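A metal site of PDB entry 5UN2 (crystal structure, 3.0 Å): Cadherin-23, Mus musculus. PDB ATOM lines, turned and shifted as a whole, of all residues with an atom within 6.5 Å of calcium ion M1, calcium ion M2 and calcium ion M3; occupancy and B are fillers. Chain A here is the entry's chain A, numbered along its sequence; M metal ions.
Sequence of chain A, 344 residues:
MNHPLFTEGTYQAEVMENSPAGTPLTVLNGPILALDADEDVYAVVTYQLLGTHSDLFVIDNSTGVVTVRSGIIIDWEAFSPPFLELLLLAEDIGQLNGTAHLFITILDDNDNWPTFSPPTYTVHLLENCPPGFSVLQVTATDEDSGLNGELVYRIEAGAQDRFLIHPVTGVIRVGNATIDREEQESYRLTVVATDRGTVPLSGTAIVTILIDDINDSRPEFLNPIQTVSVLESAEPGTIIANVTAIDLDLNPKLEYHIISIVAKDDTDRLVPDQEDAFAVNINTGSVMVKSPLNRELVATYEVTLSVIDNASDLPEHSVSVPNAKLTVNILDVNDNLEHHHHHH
CB of Ser 312 touches calcium ion M3, 3.8 Å away. His 317 touches calcium ion M3 (O to CA, 3.9 Å). Seven residues have an atom within 4 Å of calcium ion M3: Asn 215, Ser 217, Asp 247, Asp 249, Asp 309, Ser 312 and His 317. The nearest printed residue that does not touch calcium ion M3 is Arg 218 (4.3 Å).
The guanidinium group of Arg 181 sits close to the side-chain carboxylate of Asp 213 (3.2 Å). The backbone NH of Arg 181 lies close to the side-chain carboxylate of Glu 127, 3.3 Å away. The backbone NH of Ala 311 sits close to the side-chain carboxylate of Asp 309 (3.2 Å). The backbone carbonyl oxygen (O) of Asp 309 is in hydrogen-bond range of the side-chain hydroxyl (OG) of Ser 312, 3.3 Å away. The backbone NH of Leu 250 sits at hydrogen-bond distance from the side-chain carboxylate of Asp 213 (3.4 Å). The side-chain amide nitrogen of Asn 215 lies close to the backbone NH of Ser 312, at 3.4 Å. The side-chain amide nitrogen (ND2) of Asn 215 lies close to the backbone carbonyl oxygen (O) of Ala 311 (3.1 Å). OE2 of Glu 182 sits close to NH1 of Arg 181 (3.1 Å).
O of Ser 217 is bound to calcium ion M3 (2.4 Å). OD1 of Asn 215 binds calcium ion M3, 2.4 Å away. The side-chain carboxylate (OD2) of Asp 247 binds calcium ion M3. Calcium ion M3 is bound by the side-chain carboxylate (OD2) of Asp 249. The side-chain carboxylate (OD1) of Asp 247 is bound to calcium ion M3, at 2.7 Å. The side-chain carboxylate (OD2) of Asp 309 is bound to calcium ion M3, 2.7 Å away.
Calcium ion M2 is bound by the backbone carbonyl oxygen (O) of Ile 214 (2.2 Å), the side-chain carboxylate (OD1) of Asp 249 (2.4 Å), the side-chain carboxylate (OE1) of Glu 127 (2.4 Å), the side-chain carboxylate (OE2) of Glu 182 (2.4 Å), the side-chain carboxylate (OE1) of Glu 182 (2.5 Å), the side-chain carboxylate (OD1) of Asp 216 (2.6 Å) and the side-chain carboxylate (OD1) of Asp 213 (2.6 Å).
The nearest printed residue that does not touch calcium ion M2 is Asn 215 (4.3 Å).
Four residues have an atom within 4 Å of calcium ion M1: Glu 127, Asp 180, Glu 182 and Asp 216. The nearest printed residue that does not touch calcium ion M1 is Asn 128 (4.4 Å).
OD1 of Asp 180 binds calcium ion M1, at 2.3 Å. OE2 of Glu 127 is bound to calcium ion M1 (2.4 Å). OE1 of Glu 182 binds calcium ion M1. Calcium ion M1 is bound by the side-chain carboxylate (OD2) of Asp 216. The side-chain carboxylate (OD1) of Asp 216 binds calcium ion M1. Calcium ion M1 has five donor atoms within binding distance.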
ATOM      1  N   GLU A 127     -26.595  23.497 -11.782  1.00  0.00           N
ATOM      2  CA  GLU A 127     -25.369  22.727 -11.575  1.00  0.00           C
ATOM      3  C   GLU A 127     -25.014  21.944 -12.835  1.00  0.00           C
ATOM      4  O   GLU A 127     -25.848  21.815 -13.749  1.00  0.00           O
ATOM      5  CB  GLU A 127     -25.491  21.810 -10.350  1.00  0.00           C
ATOM      6  CG  GLU A 127     -26.469  20.643 -10.455  1.00  0.00           C
ATOM      7  CD  GLU A 127     -26.411  19.731  -9.237  1.00  0.00           C
ATOM      8  OE1 GLU A 127     -27.470  19.507  -8.599  1.00  0.00           O
ATOM      9  OE2 GLU A 127     -25.304  19.226  -8.895  1.00  0.00           O
ATOM     10  N   ASN A 128     -23.764  21.433 -12.885  1.00  0.00           N
ATOM     11  CA  ASN A 128     -23.179  20.753 -14.082  1.00  0.00           C
ATOM     12  C   ASN A 128     -23.174  21.634 -15.330  1.00  0.00           C
ATOM     13  O   ASN A 128     -23.229  21.106 -16.445  1.00  0.00           O
ATOM     14  CB  ASN A 128     -23.897  19.431 -14.438  1.00  0.00           C
ATOM     15  CG  ASN A 128     -24.243  18.589 -13.240  1.00  0.00           C
ATOM     16  OD1 ASN A 128     -23.477  18.479 -12.287  1.00  0.00           O
ATOM     17  ND2 ASN A 128     -25.428  17.978 -13.288  1.00  0.00           N
ATOM     18  N   ILE A 179     -19.390  22.861 -11.062  1.00  0.00           N
ATOM     19  CA  ILE A 179     -20.328  23.516 -10.118  1.00  0.00           C
ATOM     20  C   ILE A 179     -21.346  22.490  -9.594  1.00  0.00           C
ATOM     21  O   ILE A 179     -22.334  22.196 -10.270  1.00  0.00           O
ATOM     22  CB  ILE A 179     -21.086  24.721 -10.739  1.00  0.00           C
ATOM     23  CG1 ILE A 179     -20.096  25.719 -11.370  1.00  0.00           C
ATOM     24  CG2 ILE A 179     -21.992  25.392  -9.693  1.00  0.00           C
ATOM     25  CD1 ILE A 179     -18.913  26.083 -10.484  1.00  0.00           C
ATOM     26  N   ASP A 180     -21.080  21.984  -8.385  1.00  0.00           N
ATOM     27  CA  ASP A 180     -21.861  20.904  -7.760  1.00  0.00           C
ATOM     28  C   ASP A 180     -22.692  21.452  -6.611  1.00  0.00           C
ATOM     29  O   ASP A 180     -22.128  21.926  -5.621  1.00  0.00           O
ATOM     30  CB  ASP A 180     -20.902  19.830  -7.238  1.00  0.00           C
ATOM     31  CG  ASP A 180     -21.599  18.581  -6.755  1.00  0.00           C
ATOM     32  OD1 ASP A 180     -22.847  18.489  -6.870  1.00  0.00           O
ATOM     33  OD2 ASP A 180     -20.881  17.665  -6.304  1.00  0.00           O
ATOM     34  N   ARG A 181     -24.024  21.397  -6.724  1.00  0.00           N
ATOM     35  CA  ARG A 181     -24.901  21.945  -5.686  1.00  0.00           C
ATOM     36  C   ARG A 181     -24.666  21.223  -4.365  1.00  0.00           C
ATOM     37  O   ARG A 181     -24.732  21.839  -3.305  1.00  0.00           O
ATOM     38  CB  ARG A 181     -26.393  21.852  -6.063  1.00  0.00           C
ATOM     39  CG  ARG A 181     -27.289  22.833  -5.276  1.00  0.00           C
ATOM     40  CD  ARG A 181     -28.749  22.389  -5.189  1.00  0.00           C
ATOM     41  NE  ARG A 181     -28.885  21.078  -4.545  1.00  0.00           N
ATOM     42  CZ  ARG A 181     -28.972  20.840  -3.234  1.00  0.00           C
ATOM     43  NH1 ARG A 181     -29.070  19.584  -2.808  1.00  0.00           N
ATOM     44  NH2 ARG A 181     -28.971  21.825  -2.334  1.00  0.00           N
ATOM     45  N   GLU A 182     -24.362  19.936  -4.454  1.00  0.00           N
ATOM     46  CA  GLU A 182     -24.116  19.095  -3.263  1.00  0.00           C
ATOM     47  C   GLU A 182     -22.780  19.437  -2.548  1.00  0.00           C
ATOM     48  O   GLU A 182     -22.663  19.221  -1.344  1.00  0.00           O
ATOM     49  CB  GLU A 182     -24.210  17.601  -3.624  1.00  0.00           C
ATOM     50  CG  GLU A 182     -25.636  17.090  -3.868  1.00  0.00           C
ATOM     51  CD  GLU A 182     -26.330  17.647  -5.128  1.00  0.00           C
ATOM     52  OE1 GLU A 182     -25.758  17.645  -6.256  1.00  0.00           O
ATOM     53  OE2 GLU A 182     -27.499  18.063  -5.018  1.00  0.00           O
ATOM     54  N   GLU A 183     -21.808  19.971  -3.289  1.00  0.00           N
ATOM     55  CA  GLU A 183     -20.492  20.389  -2.754  1.00  0.00           C
ATOM     56  C   GLU A 183     -20.479  21.833  -2.258  1.00  0.00           C
ATOM     57  O   GLU A 183     -19.724  22.175  -1.342  1.00  0.00           O
ATOM     58  CB  GLU A 183     -19.412  20.202  -3.827  1.00  0.00           C
ATOM     59  CG  GLU A 183     -17.968  20.145  -3.320  1.00  0.00           C
ATOM     60  CD  GLU A 183     -17.218  21.471  -3.389  1.00  0.00           C
ATOM     61  OE1 GLU A 183     -16.134  21.559  -2.741  1.00  0.00           O
ATOM     62  OE2 GLU A 183     -17.696  22.406  -4.066  1.00  0.00           O
ATOM     63  N   ASP A 212     -29.003  25.972  -8.365  1.00  0.00           N
ATOM     64  CA  ASP A 212     -30.234  25.192  -8.482  1.00  0.00           C
ATOM     65  C   ASP A 212     -29.871  23.716  -8.592  1.00  0.00           C
ATOM     66  O   ASP A 212     -28.714  23.372  -8.845  1.00  0.00           O
ATOM     67  CB  ASP A 212     -31.060  25.651  -9.709  1.00  0.00           C
ATOM     68  CG  ASP A 212     -31.670  27.055  -9.522  1.00  0.00           C
ATOM     69  OD1 ASP A 212     -31.557  27.639  -8.417  1.00  0.00           O
ATOM     70  OD2 ASP A 212     -32.286  27.574 -10.479  1.00  0.00           O
ATOM     71  N   ASP A 213     -30.870  22.861  -8.408  1.00  0.00           N
ATOM     72  CA  ASP A 213     -30.685  21.407  -8.343  1.00  0.00           C
ATOM     73  C   ASP A 213     -31.031  20.673  -9.632  1.00  0.00           C
ATOM     74  O   ASP A 213     -32.060  20.918 -10.250  1.00  0.00           O
ATOM     75  CB  ASP A 213     -31.548  20.832  -7.208  1.00  0.00           C
ATOM     76  CG  ASP A 213     -31.296  19.338  -6.975  1.00  0.00           C
ATOM     77  OD1 ASP A 213     -30.156  18.964  -6.576  1.00  0.00           O
ATOM     78  OD2 ASP A 213     -32.255  18.539  -7.162  1.00  0.00           O
ATOM     79  N   ILE A 214     -30.135  19.759 -10.005  1.00  0.00           N
ATOM     80  CA  ILE A 214     -30.448  18.618 -10.847  1.00  0.00           C
ATOM     81  C   ILE A 214     -30.317  17.400  -9.931  1.00  0.00           C
ATOM     82  O   ILE A 214     -29.353  17.319  -9.142  1.00  0.00           O
ATOM     83  CB  ILE A 214     -29.443  18.498 -12.005  1.00  0.00           C
ATOM     84  CG1 ILE A 214     -29.396  19.794 -12.818  1.00  0.00           C
ATOM     85  CG2 ILE A 214     -29.781  17.315 -12.901  1.00  0.00           C
ATOM     86  CD1 ILE A 214     -28.577  19.676 -14.087  1.00  0.00           C
ATOM     87  N   ASN A 215     -31.284  16.478  -9.984  1.00  0.00           N
ATOM     88  CA  ASN A 215     -31.275  15.290  -9.119  1.00  0.00           C
ATOM     89  C   ASN A 215     -30.283  14.316  -9.715  1.00  0.00           C
ATOM     90  O   ASN A 215     -30.659  13.470 -10.529  1.00  0.00           O
ATOM     91  CB  ASN A 215     -32.695  14.704  -8.986  1.00  0.00           C
ATOM     92  CG  ASN A 215     -32.814  13.637  -7.899  1.00  0.00           C
ATOM     93  OD1 ASN A 215     -31.840  12.998  -7.509  1.00  0.00           O
ATOM     94  ND2 ASN A 215     -34.047  13.415  -7.439  1.00  0.00           N
ATOM     95  N   ASP A 216     -29.017  14.463  -9.316  1.00  0.00           N
ATOM     96  CA  ASP A 216     -27.862  13.859 -10.003  1.00  0.00           C
ATOM     97  C   ASP A 216     -26.875  13.122  -9.080  1.00  0.00           C
ATOM     98  O   ASP A 216     -25.749  12.816  -9.490  1.00  0.00           O
ATOM     99  CB  ASP A 216     -27.122  14.943 -10.806  1.00  0.00           C
ATOM    100  CG  ASP A 216     -26.383  15.956  -9.920  1.00  0.00           C
ATOM    101  OD1 ASP A 216     -26.574  15.965  -8.669  1.00  0.00           O
ATOM    102  OD2 ASP A 216     -25.576  16.757 -10.471  1.00  0.00           O
ATOM    103  N   SER A 217     -27.316  12.825  -7.864  1.00  0.00           N
ATOM    104  CA  SER A 217     -26.445  12.263  -6.818  1.00  0.00           C
ATOM    105  C   SER A 217     -27.093  11.020  -6.197  1.00  0.00           C
ATOM    106  O   SER A 217     -28.196  11.119  -5.640  1.00  0.00           O
ATOM    107  CB  SER A 217     -26.190  13.335  -5.761  1.00  0.00           C
ATOM    108  OG  SER A 217     -25.660  12.780  -4.592  1.00  0.00           O
ATOM    109  N   ARG A 218     -26.412   9.881  -6.314  1.00  0.00           N
ATOM    110  CA  ARG A 218     -26.995   8.585  -5.935  1.00  0.00           C
ATOM    111  C   ARG A 218     -27.242   8.472  -4.436  1.00  0.00           C
ATOM    112  O   ARG A 218     -26.465   9.016  -3.643  1.00  0.00           O
ATOM    113  CB  ARG A 218     -26.119   7.409  -6.407  1.00  0.00           C
ATOM    114  CG  ARG A 218     -24.828   7.211  -5.602  1.00  0.00           C
ATOM    115  CD  ARG A 218     -24.044   5.983  -6.038  1.00  0.00           C
ATOM    116  NE  ARG A 218     -23.458   6.170  -7.356  1.00  0.00           N
ATOM    117  CZ  ARG A 218     -23.982   5.758  -8.501  1.00  0.00           C
ATOM    118  NH1 ARG A 218     -23.311   6.028  -9.628  1.00  0.00           N
ATOM    119  NH2 ARG A 218     -25.137   5.083  -8.561  1.00  0.00           N
ATOM    120  N   PRO A 219     -28.310   7.758  -4.048  1.00  0.00           N
ATOM    121  CA  PRO A 219     -28.503   7.524  -2.618  1.00  0.00           C
ATOM    122  C   PRO A 219     -27.340   6.720  -2.013  1.00  0.00           C
ATOM    123  O   PRO A 219     -26.695   5.905  -2.704  1.00  0.00           O
ATOM    124  CB  PRO A 219     -29.808   6.743  -2.561  1.00  0.00           C
ATOM    125  CG  PRO A 219     -29.870   6.046  -3.873  1.00  0.00           C
ATOM    126  CD  PRO A 219     -29.315   7.039  -4.848  1.00  0.00           C
ATOM    127  N   ASP A 247     -29.969  10.656   0.125  1.00  0.00           N
ATOM    128  CA  ASP A 247     -29.742  11.268  -1.188  1.00  0.00           C
ATOM    129  C   ASP A 247     -29.560  12.770  -0.911  1.00  0.00           C
ATOM    130  O   ASP A 247     -30.389  13.385  -0.247  1.00  0.00           O
ATOM    131  CB  ASP A 247     -30.977  11.008  -2.097  1.00  0.00           C
ATOM    132  CG  ASP A 247     -30.718  11.233  -3.627  1.00  0.00           C
ATOM    133  OD1 ASP A 247     -30.739  12.372  -4.133  1.00  0.00           O
ATOM    134  OD2 ASP A 247     -30.559  10.225  -4.365  1.00  0.00           O
ATOM    135  N   LEU A 248     -28.473  13.361  -1.393  1.00  0.00           N
ATOM    136  CA  LEU A 248     -28.180  14.759  -1.049  1.00  0.00           C
ATOM    137  C   LEU A 248     -28.851  15.756  -1.986  1.00  0.00           C
ATOM    138  O   LEU A 248     -28.645  16.955  -1.825  1.00  0.00           O
ATOM    139  CB  LEU A 248     -26.664  15.014  -1.004  1.00  0.00           C
ATOM    140  CG  LEU A 248     -25.852  14.072  -0.108  1.00  0.00           C
ATOM    141  CD1 LEU A 248     -24.359  14.247  -0.290  1.00  0.00           C
ATOM    142  CD2 LEU A 248     -26.227  14.245   1.356  1.00  0.00           C
ATOM    143  N   ASP A 249     -29.650  15.267  -2.948  1.00  0.00           N
ATOM    144  CA  ASP A 249     -30.384  16.145  -3.897  1.00  0.00           C
ATOM    145  C   ASP A 249     -31.632  16.731  -3.240  1.00  0.00           C
ATOM    146  O   ASP A 249     -31.991  16.337  -2.130  1.00  0.00           O
ATOM    147  CB  ASP A 249     -30.783  15.383  -5.160  1.00  0.00           C
ATOM    148  CG  ASP A 249     -29.611  14.823  -5.901  1.00  0.00           C
ATOM    149  OD1 ASP A 249     -28.728  15.621  -6.250  1.00  0.00           O
ATOM    150  OD2 ASP A 249     -29.584  13.600  -6.148  1.00  0.00           O
ATOM    151  N   LEU A 250     -32.311  17.625  -3.938  1.00  0.00           N
ATOM    152  CA  LEU A 250     -33.320  18.461  -3.290  1.00  0.00           C
ATOM    153  C   LEU A 250     -34.657  17.786  -2.975  1.00  0.00           C
ATOM    154  O   LEU A 250     -35.270  18.095  -1.948  1.00  0.00           O
ATOM    155  CB  LEU A 250     -33.537  19.753  -4.067  1.00  0.00           C
ATOM    156  CG  LEU A 250     -33.615  21.023  -3.222  1.00  0.00           C
ATOM    157  CD1 LEU A 250     -32.356  21.207  -2.381  1.00  0.00           C
ATOM    158  CD2 LEU A 250     -33.852  22.222  -4.137  1.00  0.00           C
ATOM    159  N   PRO A 252     -35.770  13.975  -3.150  1.00  0.00           N
ATOM    160  CA  PRO A 252     -35.642  12.552  -3.491  1.00  0.00           C
ATOM    161  C   PRO A 252     -36.905  11.787  -3.210  1.00  0.00           C
ATOM    162  O   PRO A 252     -37.679  12.192  -2.365  1.00  0.00           O
ATOM    163  CB  PRO A 252     -34.521  12.065  -2.567  1.00  0.00           C
ATOM    164  CG  PRO A 252     -34.050  13.249  -1.802  1.00  0.00           C
ATOM    165  CD  PRO A 252     -35.134  14.268  -1.864  1.00  0.00           C
ATOM    166  N   LEU A 254     -36.979   8.097  -2.275  1.00  0.00           N
ATOM    167  CA  LEU A 254     -36.269   6.843  -2.053  1.00  0.00           C
ATOM    168  C   LEU A 254     -37.187   5.646  -1.962  1.00  0.00           C
ATOM    169  O   LEU A 254     -38.252   5.712  -1.374  1.00  0.00           O
ATOM    170  CB  LEU A 254     -35.386   6.907  -0.813  1.00  0.00           C
ATOM    171  CG  LEU A 254     -33.958   7.429  -1.035  1.00  0.00           C
ATOM    172  CD1 LEU A 254     -33.970   8.707  -1.867  1.00  0.00           C
ATOM    173  CD2 LEU A 254     -33.256   7.659   0.300  1.00  0.00           C
ATOM    174  N   ASP A 309     -33.335   6.416  -6.028  1.00  0.00           N
ATOM    175  CA  ASP A 309     -34.034   7.691  -6.081  1.00  0.00           C
ATOM    176  C   ASP A 309     -34.875   7.766  -7.375  1.00  0.00           C
ATOM    177  O   ASP A 309     -34.325   8.015  -8.448  1.00  0.00           O
ATOM    178  CB  ASP A 309     -33.042   8.860  -6.007  1.00  0.00           C
ATOM    179  CG  ASP A 309     -33.717  10.217  -5.797  1.00  0.00           C
ATOM    180  OD1 ASP A 309     -34.970  10.253  -5.762  1.00  0.00           O
ATOM    181  OD2 ASP A 309     -32.991  11.229  -5.648  1.00  0.00           O
ATOM    182  N   ALA A 311     -36.849  10.017  -8.302  1.00  0.00           N
ATOM    183  CA  ALA A 311     -36.823  11.363  -8.847  1.00  0.00           C
ATOM    184  C   ALA A 311     -35.530  11.693  -9.597  1.00  0.00           C
ATOM    185  O   ALA A 311     -35.447  12.771 -10.182  1.00  0.00           O
ATOM    186  CB  ALA A 311     -37.053  12.378  -7.740  1.00  0.00           C
ATOM    187  N   SER A 312     -34.525  10.810  -9.596  1.00  0.00           N
ATOM    188  CA  SER A 312     -33.219  11.187 -10.139  1.00  0.00           C
ATOM    189  C   SER A 312     -33.269  11.482 -11.656  1.00  0.00           C
ATOM    190  O   SER A 312     -33.856  10.734 -12.445  1.00  0.00           O
ATOM    191  CB  SER A 312     -32.103  10.188  -9.794  1.00  0.00           C
ATOM    192  OG  SER A 312     -32.082   9.088 -10.688  1.00  0.00           O
ATOM    193  N   ASP A 313     -32.669  12.618 -12.019  1.00  0.00           N
ATOM    194  CA  ASP A 313     -32.664  13.100 -13.384  1.00  0.00           C
ATOM    195  C   ASP A 313     -31.591  12.344 -14.192  1.00  0.00           C
ATOM    196  O   ASP A 313     -31.729  12.226 -15.378  1.00  0.00           O
ATOM    197  CB  ASP A 313     -32.439  14.625 -13.435  1.00  0.00           C
ATOM    198  CG  ASP A 313     -33.623  15.444 -12.845  1.00  0.00           C
ATOM    199  OD1 ASP A 313     -34.797  15.201 -13.191  1.00  0.00           O
ATOM    200  OD2 ASP A 313     -33.383  16.374 -12.033  1.00  0.00           O
ATOM    201  N   HIS A 317     -26.937   7.612 -11.694  1.00  0.00           N
ATOM    202  CA  HIS A 317     -26.877   7.950 -10.252  1.00  0.00           C
ATOM    203  C   HIS A 317     -28.223   7.741  -9.564  1.00  0.00           C
ATOM    204  O   HIS A 317     -28.716   8.593  -8.788  1.00  0.00           O
ATOM    205  CB  HIS A 317     -26.415   9.387 -10.101  1.00  0.00           C
ATOM    206  CG  HIS A 317     -25.107   9.649 -10.752  1.00  0.00           C
ATOM    207  ND1 HIS A 317     -23.901   9.461 -10.113  1.00  0.00           N
ATOM    208  CD2 HIS A 317     -24.803  10.084 -12.002  1.00  0.00           C
ATOM    209  CE1 HIS A 317     -22.916   9.769 -10.934  1.00  0.00           C
ATOM    210  NE2 HIS A 317     -23.442  10.144 -12.089  1.00  0.00           N
ATOM    211  N   SER A 318     -28.828   6.598  -9.881  1.00  0.00           N
ATOM    212  CA  SER A 318     -30.164   6.267  -9.431  1.00  0.00           C
ATOM    213  C   SER A 318     -30.110   5.424  -8.189  1.00  0.00           C
ATOM    214  O   SER A 318     -30.878   5.635  -7.256  1.00  0.00           O
ATOM    215  CB  SER A 318     -30.888   5.462 -10.498  1.00  0.00           C
ATOM    216  OG  SER A 318     -31.231   6.282 -11.580  1.00  0.00           O
HETATM  217 CA    CA M   1     -24.251  17.233  -8.186  1.00  0.00          CA
HETATM  218 CA    CA M   2     -28.051  17.595  -7.338  1.00  0.00          CA
HETATM  219 CA    CA M   3     -30.416  11.303  -6.537  1.00  0.00          CA
